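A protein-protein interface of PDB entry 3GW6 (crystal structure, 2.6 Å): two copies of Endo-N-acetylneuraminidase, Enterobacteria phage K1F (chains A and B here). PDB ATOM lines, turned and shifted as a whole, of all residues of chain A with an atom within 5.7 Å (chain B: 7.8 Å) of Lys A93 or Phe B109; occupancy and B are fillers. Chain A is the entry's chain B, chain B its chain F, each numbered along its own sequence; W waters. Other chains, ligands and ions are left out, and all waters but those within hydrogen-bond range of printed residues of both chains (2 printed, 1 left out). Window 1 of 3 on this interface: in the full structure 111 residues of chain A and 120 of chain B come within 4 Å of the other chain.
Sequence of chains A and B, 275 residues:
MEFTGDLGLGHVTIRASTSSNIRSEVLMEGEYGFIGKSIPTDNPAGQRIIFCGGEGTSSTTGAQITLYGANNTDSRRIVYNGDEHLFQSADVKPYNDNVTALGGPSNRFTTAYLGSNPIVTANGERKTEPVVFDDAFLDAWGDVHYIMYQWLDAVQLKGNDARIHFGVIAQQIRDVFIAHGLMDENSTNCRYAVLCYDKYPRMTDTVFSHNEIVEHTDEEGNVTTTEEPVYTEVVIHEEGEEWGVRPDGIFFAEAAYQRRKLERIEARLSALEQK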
ATOM      1  N   ASP A  91     -21.515  24.286   7.215  1.00  0.00           N
ATOM      2  CA  ASP A  91     -20.696  23.530   8.146  1.00  0.00           C
ATOM      3  C   ASP A  91     -19.909  24.471   9.053  1.00  0.00           C
ATOM      4  O   ASP A  91     -19.604  25.603   8.678  1.00  0.00           O
ATOM      5  CB  ASP A  91     -19.718  22.630   7.384  1.00  0.00           C
ATOM      6  CG  ASP A  91     -20.397  21.803   6.307  1.00  0.00           C
ATOM      7  OD1 ASP A  91     -21.539  21.349   6.530  1.00  0.00           O
ATOM      8  OD2 ASP A  91     -19.782  21.603   5.235  1.00  0.00           O
ATOM      9  N   VAL A  92     -19.587  24.003  10.253  1.00  0.00           N
ATOM     10  CA  VAL A  92     -18.652  24.718  11.104  1.00  0.00           C
ATOM     11  C   VAL A  92     -17.260  24.186  10.809  1.00  0.00           C
ATOM     12  O   VAL A  92     -16.918  23.067  11.189  1.00  0.00           O
ATOM     13  CB  VAL A  92     -18.984  24.558  12.594  1.00  0.00           C
ATOM     14  CG1 VAL A  92     -17.912  25.227  13.451  1.00  0.00           C
ATOM     15  CG2 VAL A  92     -20.355  25.142  12.887  1.00  0.00           C
ATOM     16  N   LYS A  93     -16.467  24.992  10.108  1.00  0.00           N
ATOM     17  CA  LYS A  93     -15.176  24.548   9.600  1.00  0.00           C
ATOM     18  C   LYS A  93     -13.995  25.328  10.165  1.00  0.00           C
ATOM     19  O   LYS A  93     -14.136  26.480  10.585  1.00  0.00           O
ATOM     20  CB  LYS A  93     -15.144  24.677   8.077  1.00  0.00           C
ATOM     21  CG  LYS A  93     -15.922  23.609   7.326  1.00  0.00           C
ATOM     22  CD  LYS A  93     -15.760  23.815   5.831  1.00  0.00           C
ATOM     23  CE  LYS A  93     -16.589  22.833   5.029  1.00  0.00           C
ATOM     24  NZ  LYS A  93     -16.580  23.198   3.586  1.00  0.00           N
ATOM     25  N   PRO A  94     -12.811  24.697  10.160  1.00  0.00           N
ATOM     26  CA  PRO A  94     -11.568  25.429  10.394  1.00  0.00           C
ATOM     27  C   PRO A  94     -11.233  26.229   9.141  1.00  0.00           C
ATOM     28  O   PRO A  94     -11.615  25.830   8.038  1.00  0.00           O
ATOM     29  CB  PRO A  94     -10.530  24.316  10.585  1.00  0.00           C
ATOM     30  CG  PRO A  94     -11.305  23.020  10.650  1.00  0.00           C
ATOM     31  CD  PRO A  94     -12.573  23.267   9.913  1.00  0.00           C
ATOM     32  N   TYR A  95     -10.532  27.343   9.297  1.00  0.00           N
ATOM     33  CA  TYR A  95     -10.091  28.103   8.137  1.00  0.00           C
ATOM     34  C   TYR A  95      -9.155  27.246   7.289  1.00  0.00           C
ATOM     35  O   TYR A  95      -9.392  27.028   6.098  1.00  0.00           O
ATOM     36  CB  TYR A  95      -9.379  29.374   8.580  1.00  0.00           C
ATOM     37  CG  TYR A  95      -9.028  30.318   7.459  1.00  0.00           C
ATOM     38  CD1 TYR A  95      -9.891  31.342   7.093  1.00  0.00           C
ATOM     39  CD2 TYR A  95      -7.827  30.195   6.773  1.00  0.00           C
ATOM     40  CE1 TYR A  95      -9.568  32.214   6.073  1.00  0.00           C
ATOM     41  CE2 TYR A  95      -7.500  31.066   5.754  1.00  0.00           C
ATOM     42  CZ  TYR A  95      -8.373  32.071   5.410  1.00  0.00           C
ATOM     43  OH  TYR A  95      -8.048  32.940   4.393  1.00  0.00           O
ATOM     44  N   ASN A  98      -6.318  20.926   8.767  1.00  0.00           N
ATOM     45  CA  ASN A  98      -5.535  20.134   9.712  1.00  0.00           C
ATOM     46  C   ASN A  98      -4.485  20.938  10.476  1.00  0.00           C
ATOM     47  O   ASN A  98      -3.352  20.486  10.635  1.00  0.00           O
ATOM     48  CB  ASN A  98      -4.865  18.967   8.980  1.00  0.00           C
ATOM     49  CG  ASN A  98      -4.370  17.887   9.920  1.00  0.00           C
ATOM     50  OD1 ASN A  98      -5.047  17.529  10.883  1.00  0.00           O
ATOM     51  ND2 ASN A  98      -3.190  17.351   9.637  1.00  0.00           N
ATOM     52  N   VAL A  99      -4.862  22.123  10.946  1.00  0.00           N
ATOM     53  CA  VAL A  99      -3.953  22.955  11.732  1.00  0.00           C
ATOM     54  C   VAL A  99      -4.519  23.298  13.111  1.00  0.00           C
ATOM     55  O   VAL A  99      -3.776  23.393  14.086  1.00  0.00           O
ATOM     56  CB  VAL A  99      -3.588  24.263  11.004  1.00  0.00           C
ATOM     57  CG1 VAL A  99      -2.686  23.981   9.811  1.00  0.00           C
ATOM     58  CG2 VAL A  99      -4.842  24.991  10.569  1.00  0.00           C
ATOM     59  N   THR A 100      -5.833  23.490  13.187  1.00  0.00           N
ATOM     60  CA  THR A 100      -6.485  23.815  14.451  1.00  0.00           C
ATOM     61  C   THR A 100      -7.508  22.749  14.836  1.00  0.00           C
ATOM     62  O   THR A 100      -7.961  21.977  13.991  1.00  0.00           O
ATOM     63  CB  THR A 100      -7.158  25.200  14.406  1.00  0.00           C
ATOM     64  OG1 THR A 100      -8.343  25.135  13.603  1.00  0.00           O
ATOM     65  CG2 THR A 100      -6.206  26.231  13.820  1.00  0.00           C
ATOM     66  N   ALA A 101      -7.881  22.718  16.112  1.00  0.00           N
ATOM     67  CA  ALA A 101      -8.675  21.613  16.640  1.00  0.00           C
ATOM     68  C   ALA A 101      -9.978  22.051  17.289  1.00  0.00           C
ATOM     69  O   ALA A 101     -10.195  23.232  17.543  1.00  0.00           O
ATOM     70  CB  ALA A 101      -7.853  20.808  17.631  1.00  0.00           C
ATOM     71  N   LEU A 102     -10.840  21.075  17.551  1.00  0.00           N
ATOM     72  CA  LEU A 102     -12.032  21.287  18.357  1.00  0.00           C
ATOM     73  C   LEU A 102     -11.697  20.979  19.812  1.00  0.00           C
ATOM     74  O   LEU A 102     -11.223  19.886  20.127  1.00  0.00           O
ATOM     75  CB  LEU A 102     -13.170  20.380  17.882  1.00  0.00           C
ATOM     76  CG  LEU A 102     -13.925  20.786  16.615  1.00  0.00           C
ATOM     77  CD1 LEU A 102     -14.696  19.605  16.041  1.00  0.00           C
ATOM     78  CD2 LEU A 102     -14.857  21.956  16.896  1.00  0.00           C
ATOM     79  N   ILE B  78     -18.405  33.858   6.213  1.00  0.00           N
ATOM     80  CA  ILE B  78     -18.011  34.493   7.462  1.00  0.00           C
ATOM     81  C   ILE B  78     -16.616  34.021   7.845  1.00  0.00           C
ATOM     82  O   ILE B  78     -16.298  32.839   7.735  1.00  0.00           O
ATOM     83  CB  ILE B  78     -18.981  34.207   8.622  1.00  0.00           C
ATOM     84  CG1 ILE B  78     -20.399  34.657   8.269  1.00  0.00           C
ATOM     85  CG2 ILE B  78     -18.517  34.921   9.879  1.00  0.00           C
ATOM     86  CD1 ILE B  78     -21.397  34.468   9.397  1.00  0.00           C
ATOM     87  N   TYR B  80     -13.916  34.163  11.018  1.00  0.00           N
ATOM     88  CA  TYR B  80     -13.616  34.480  12.408  1.00  0.00           C
ATOM     89  C   TYR B  80     -12.113  34.391  12.617  1.00  0.00           C
ATOM     90  O   TYR B  80     -11.548  33.301  12.600  1.00  0.00           O
ATOM     91  CB  TYR B  80     -14.317  33.504  13.359  1.00  0.00           C
ATOM     92  CG  TYR B  80     -15.773  33.239  13.046  1.00  0.00           C
ATOM     93  CD1 TYR B  80     -16.786  33.846  13.779  1.00  0.00           C
ATOM     94  CD2 TYR B  80     -16.135  32.371  12.021  1.00  0.00           C
ATOM     95  CE1 TYR B  80     -18.117  33.599  13.496  1.00  0.00           C
ATOM     96  CE2 TYR B  80     -17.462  32.121  11.729  1.00  0.00           C
ATOM     97  CZ  TYR B  80     -18.448  32.734  12.469  1.00  0.00           C
ATOM     98  OH  TYR B  80     -19.771  32.486  12.183  1.00  0.00           O
ATOM     99  N   ALA B 101     -22.053  20.065   8.832  1.00  0.00           N
ATOM    100  CA  ALA B 101     -20.996  19.226   9.382  1.00  0.00           C
ATOM    101  C   ALA B 101     -19.938  19.999  10.158  1.00  0.00           C
ATOM    102  O   ALA B 101     -19.796  21.209  10.009  1.00  0.00           O
ATOM    103  CB  ALA B 101     -20.335  18.433   8.265  1.00  0.00           C
ATOM    104  N   LEU B 102     -19.197  19.274  10.989  1.00  0.00           N
ATOM    105  CA  LEU B 102     -18.000  19.797  11.628  1.00  0.00           C
ATOM    106  C   LEU B 102     -16.796  19.482  10.752  1.00  0.00           C
ATOM    107  O   LEU B 102     -16.492  18.318  10.497  1.00  0.00           O
ATOM    108  CB  LEU B 102     -17.813  19.170  13.011  1.00  0.00           C
ATOM    109  CG  LEU B 102     -18.568  19.831  14.170  1.00  0.00           C
ATOM    110  CD1 LEU B 102     -18.580  18.926  15.392  1.00  0.00           C
ATOM    111  CD2 LEU B 102     -17.973  21.191  14.509  1.00  0.00           C
ATOM    112  N   GLY B 103     -16.115  20.520  10.281  1.00  0.00           N
ATOM    113  CA  GLY B 103     -14.966  20.331   9.417  1.00  0.00           C
ATOM    114  C   GLY B 103     -15.357  19.922   8.010  1.00  0.00           C
ATOM    115  O   GLY B 103     -16.533  19.960   7.644  1.00  0.00           O
ATOM    116  N   GLY B 104     -14.366  19.532   7.216  1.00  0.00           N
ATOM    117  CA  GLY B 104     -14.612  19.114   5.849  1.00  0.00           C
ATOM    118  C   GLY B 104     -13.415  18.414   5.248  1.00  0.00           C
ATOM    119  O   GLY B 104     -12.349  18.368   5.864  1.00  0.00           O
ATOM    120  N   PRO B 105     -13.584  17.861   4.035  1.00  0.00           N
ATOM    121  CA  PRO B 105     -12.523  17.143   3.324  1.00  0.00           C
ATOM    122  C   PRO B 105     -11.230  17.949   3.254  1.00  0.00           C
ATOM    123  O   PRO B 105     -10.147  17.393   3.437  1.00  0.00           O
ATOM    124  CB  PRO B 105     -13.105  16.969   1.919  1.00  0.00           C
ATOM    125  CG  PRO B 105     -14.572  16.948   2.131  1.00  0.00           C
ATOM    126  CD  PRO B 105     -14.836  17.901   3.257  1.00  0.00           C
ATOM    127  N   SER B 106     -11.345  19.247   2.997  1.00  0.00           N
ATOM    128  CA  SER B 106     -10.171  20.100   2.874  1.00  0.00           C
ATOM    129  C   SER B 106     -10.119  21.138   3.993  1.00  0.00           C
ATOM    130  O   SER B 106      -9.278  22.039   3.982  1.00  0.00           O
ATOM    131  CB  SER B 106     -10.145  20.784   1.509  1.00  0.00           C
ATOM    132  OG  SER B 106      -8.855  21.295   1.231  1.00  0.00           O
ATOM    133  N   ASN B 107     -11.033  21.006   4.947  1.00  0.00           N
ATOM    134  CA  ASN B 107     -11.027  21.836   6.146  1.00  0.00           C
ATOM    135  C   ASN B 107     -11.162  20.963   7.390  1.00  0.00           C
ATOM    136  O   ASN B 107     -12.163  21.023   8.100  1.00  0.00           O
ATOM    137  CB  ASN B 107     -12.149  22.875   6.097  1.00  0.00           C
ATOM    138  CG  ASN B 107     -12.086  23.741   4.855  1.00  0.00           C
ATOM    139  OD1 ASN B 107     -11.705  24.910   4.920  1.00  0.00           O
ATOM    140  ND2 ASN B 107     -12.448  23.169   3.714  1.00  0.00           N
ATOM    141  N   ARG B 108     -10.146  20.145   7.638  1.00  0.00           N
ATOM    142  CA  ARG B 108     -10.174  19.186   8.731  1.00  0.00           C
ATOM    143  C   ARG B 108      -9.763  19.818  10.051  1.00  0.00           C
ATOM    144  O   ARG B 108      -8.888  20.685  10.095  1.00  0.00           O
ATOM    145  CB  ARG B 108      -9.235  18.014   8.431  1.00  0.00           C
ATOM    146  CG  ARG B 108      -9.537  17.262   7.144  1.00  0.00           C
ATOM    147  CD  ARG B 108      -8.424  16.277   6.829  1.00  0.00           C
ATOM    148  NE  ARG B 108      -7.246  16.947   6.287  1.00  0.00           N
ATOM    149  CZ  ARG B 108      -6.000  16.509   6.436  1.00  0.00           C
ATOM    150  NH1 ARG B 108      -5.761  15.405   7.129  1.00  0.00           N
ATOM    151  NH2 ARG B 108      -4.990  17.184   5.905  1.00  0.00           N
ATOM    152  N   PHE B 109     -10.399  19.376  11.128  1.00  0.00           N
ATOM    153  CA  PHE B 109      -9.922  19.693  12.463  1.00  0.00           C
ATOM    154  C   PHE B 109      -8.901  18.631  12.836  1.00  0.00           C
ATOM    155  O   PHE B 109      -9.096  17.451  12.546  1.00  0.00           O
ATOM    156  CB  PHE B 109     -11.069  19.692  13.472  1.00  0.00           C
ATOM    157  CG  PHE B 109     -11.919  20.929  13.430  1.00  0.00           C
ATOM    158  CD1 PHE B 109     -11.409  22.152  13.834  1.00  0.00           C
ATOM    159  CD2 PHE B 109     -13.235  20.868  13.002  1.00  0.00           C
ATOM    160  CE1 PHE B 109     -12.191  23.292  13.805  1.00  0.00           C
ATOM    161  CE2 PHE B 109     -14.024  22.003  12.970  1.00  0.00           C
ATOM    162  CZ  PHE B 109     -13.499  23.219  13.370  1.00  0.00           C
ATOM    163  N   THR B 110      -7.805  19.042  13.464  1.00  0.00           N
ATOM    164  CA  THR B 110      -6.773  18.087  13.854  1.00  0.00           C
ATOM    165  C   THR B 110      -7.374  17.005  14.740  1.00  0.00           C
ATOM    166  O   THR B 110      -7.129  15.818  14.538  1.00  0.00           O
ATOM    167  CB  THR B 110      -5.608  18.766  14.591  1.00  0.00           C
ATOM    168  OG1 THR B 110      -6.112  19.488  15.720  1.00  0.00           O
ATOM    169  CG2 THR B 110      -4.879  19.726  13.665  1.00  0.00           C
ATOM    170  N   THR B 111      -8.168  17.422  15.720  1.00  0.00           N
ATOM    171  CA  THR B 111      -8.852  16.475  16.588  1.00  0.00           C
ATOM    172  C   THR B 111     -10.035  17.143  17.263  1.00  0.00           C
ATOM    173  O   THR B 111     -10.339  18.304  17.003  1.00  0.00           O
ATOM    174  CB  THR B 111      -7.926  15.949  17.698  1.00  0.00           C
ATOM    175  OG1 THR B 111      -6.557  16.153  17.330  1.00  0.00           O
ATOM    176  CG2 THR B 111      -8.175  14.473  17.935  1.00  0.00           C
ATOM    177  N   ALA B 112     -10.696  16.391  18.135  1.00  0.00           N
ATOM    178  CA  ALA B 112     -11.702  16.939  19.028  1.00  0.00           C
ATOM    179  C   ALA B 112     -11.352  16.505  20.443  1.00  0.00           C
ATOM    180  O   ALA B 112     -11.095  15.327  20.686  1.00  0.00           O
ATOM    181  CB  ALA B 112     -13.086  16.455  18.644  1.00  0.00           C
ATOM    182  N   TYR B 200     -13.008  18.105  -3.890  1.00  0.00           N
ATOM    183  CA  TYR B 200     -13.200  19.451  -3.348  1.00  0.00           C
ATOM    184  C   TYR B 200     -12.571  20.572  -4.177  1.00  0.00           C
ATOM    185  O   TYR B 200     -11.496  20.403  -4.756  1.00  0.00           O
ATOM    186  CB  TYR B 200     -12.730  19.528  -1.890  1.00  0.00           C
ATOM    187  CG  TYR B 200     -11.277  19.177  -1.667  1.00  0.00           C
ATOM    188  CD1 TYR B 200     -10.917  17.990  -1.044  1.00  0.00           C
ATOM    189  CD2 TYR B 200     -10.267  20.036  -2.067  1.00  0.00           C
ATOM    190  CE1 TYR B 200      -9.591  17.669  -0.834  1.00  0.00           C
ATOM    191  CE2 TYR B 200      -8.941  19.724  -1.860  1.00  0.00           C
ATOM    192  CZ  TYR B 200      -8.608  18.541  -1.244  1.00  0.00           C
ATOM    193  OH  TYR B 200      -7.282  18.239  -1.039  1.00  0.00           O
ATOM    194  N   PRO B 201     -13.254  21.724  -4.226  1.00  0.00           N
ATOM    195  CA  PRO B 201     -12.821  22.911  -4.970  1.00  0.00           C
ATOM    196  C   PRO B 201     -11.611  23.564  -4.321  1.00  0.00           C
ATOM    197  O   PRO B 201     -11.248  23.219  -3.194  1.00  0.00           O
ATOM    198  CB  PRO B 201     -14.029  23.852  -4.869  1.00  0.00           C
ATOM    199  CG  PRO B 201     -15.167  23.011  -4.366  1.00  0.00           C
ATOM    200  CD  PRO B 201     -14.537  21.942  -3.540  1.00  0.00           C
ATOM    201  N   MET B 203      -9.742  26.844  -2.618  1.00  0.00           N
ATOM    202  CA  MET B 203     -10.226  27.871  -1.702  1.00  0.00           C
ATOM    203  C   MET B 203      -9.407  29.155  -1.780  1.00  0.00           C
ATOM    204  O   MET B 203      -8.208  29.160  -1.500  1.00  0.00           O
ATOM    205  CB  MET B 203     -10.241  27.349  -0.264  1.00  0.00           C
ATOM    206  CG  MET B 203     -10.337  28.438   0.791  1.00  0.00           C
ATOM    207  SD  MET B 203     -10.382  27.774   2.467  1.00  0.00           S
ATOM    208  CE  MET B 203     -10.059  29.252   3.422  1.00  0.00           C
HETATM  209  O   HOH W   1      -8.037  24.992   3.957  1.00  0.00           O
HETATM  210  O   HOH W   2     -17.985  19.213   4.636  1.00  0.00           O
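O of Tyr A95 lies close to OD1 of Asn B107. The backbone NH (N) of Thr B110 lies within hydrogen-bond range of the backbone carbonyl oxygen (O) of Thr A100 (3.0 Å). N of Ala B101 lies within hydrogen-bond range of OD1 of Asp A91 (2.7 Å). The backbone NH of Leu A102 lies within hydrogen-bond range of the backbone carbonyl oxygen of Thr B111 (2.9 Å). The backbone carbonyl oxygen (O) of Arg B108 is in hydrogen-bond range of the backbone NH (N) of Asn A98 (2.9 Å). The backbone NH of Gly B103 sits at hydrogen-bond distance from the backbone carbonyl oxygen of Val A92, at 2.8 Å. N of Val A92 is in hydrogen-bond range of O of Ala B101. OD1 of Asn B107 sits close to O of Pro A94 (3.3 Å).
OD2 of Asp A91 lies within salt-bridge range of NZ of Lys A93 (3.9 Å).
Leu B102 touches Val A92. Phe B109 touches Val A92 (CE2 to O, 3.6 Å). O of Gly B103 touches CG of Lys A93, at 3.7 Å. C of Lys A93 touches CZ of Phe B109, at 3.9 Å. CD of Pro A94 touches CA of Gly B103 (3.8 Å). Pro A94 touches Arg B108 (CG to O, 3.4 Å). Thr B110 touches Val A99 (CG2 to N, 3.6 Å). Ala A101 touches Phe B109 (C to CD1, 3.7 Å). OG1 of Thr B110 touches CB of Ala A101 (2.9 Å). Leu A102 touches Leu B102 (CD1 to CD2, 3.9 Å).
Of chain B, only Gly B103 (3.7 Å), Asn B107 (3.7 Å) and Phe B109 (3.9 Å) come within 4 Å of Lys A93. Phe B109 touches just these residues of chain A: Val A92, Lys A93, Pro A94, Thr A100, Ala A101 and Leu A102. Pro A94 touches four residues of chain B. Printed residues of chain A within 4 Å of Leu B102: Val A92 and Leu A102. Printed residues of chain B within 4 Å of Asp A91: Ala B101. Of the printed residues of chain B, Asn A98 touches Arg B108 and Thr B110. Printed residues of chain B within 4 Å of Leu A102: Leu B102, Phe B109, Thr B111 and Ala B112. Printed residues of chain B within 4 Å of Thr A100: Phe B109 (3.4 Å) and Thr B110 (3.0 Å). Ser B106 touches none of the printed residues of chain A. The nearest residue of chain B that does not touch Lys A93 is Gly B104 (4.3 Å). The nearest residue of chain A that does not touch Phe B109 is Asn A98 (4.4 Å). The nearest printed residue of chain B that does not touch Val A99 is Arg B108 (4.4 Å).
Hydrophobic or aromatic side chains of chain B that line the printed part of chain A: Ala B101, Leu B102, Phe B109, Ala B112 and Met B203. Printed residues of chain A that touch a printed residue of chain B: Asp A91, Val A92, Lys A93, Pro A94, Tyr A95, Asn A98, Val A99, Thr A100, Ala A101 and Leu A102.
Leu A102 touches its own counterpart, Leu B102. Of the 26 pairs that touch across the chains among the printed residues, 1 has its exchanged pair printed and touching as well.
Water W2 lies within hydrogen-bond range of the side-chain carboxylate (OD2) of Asp A91 (3.0 Å) and the backbone carbonyl oxygen (O) of Gly B103 (3.4 Å). Water W1 lies within hydrogen-bond range of O of Ser B106 (3.2 Å) and O of Tyr A95 (3.3 Å).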
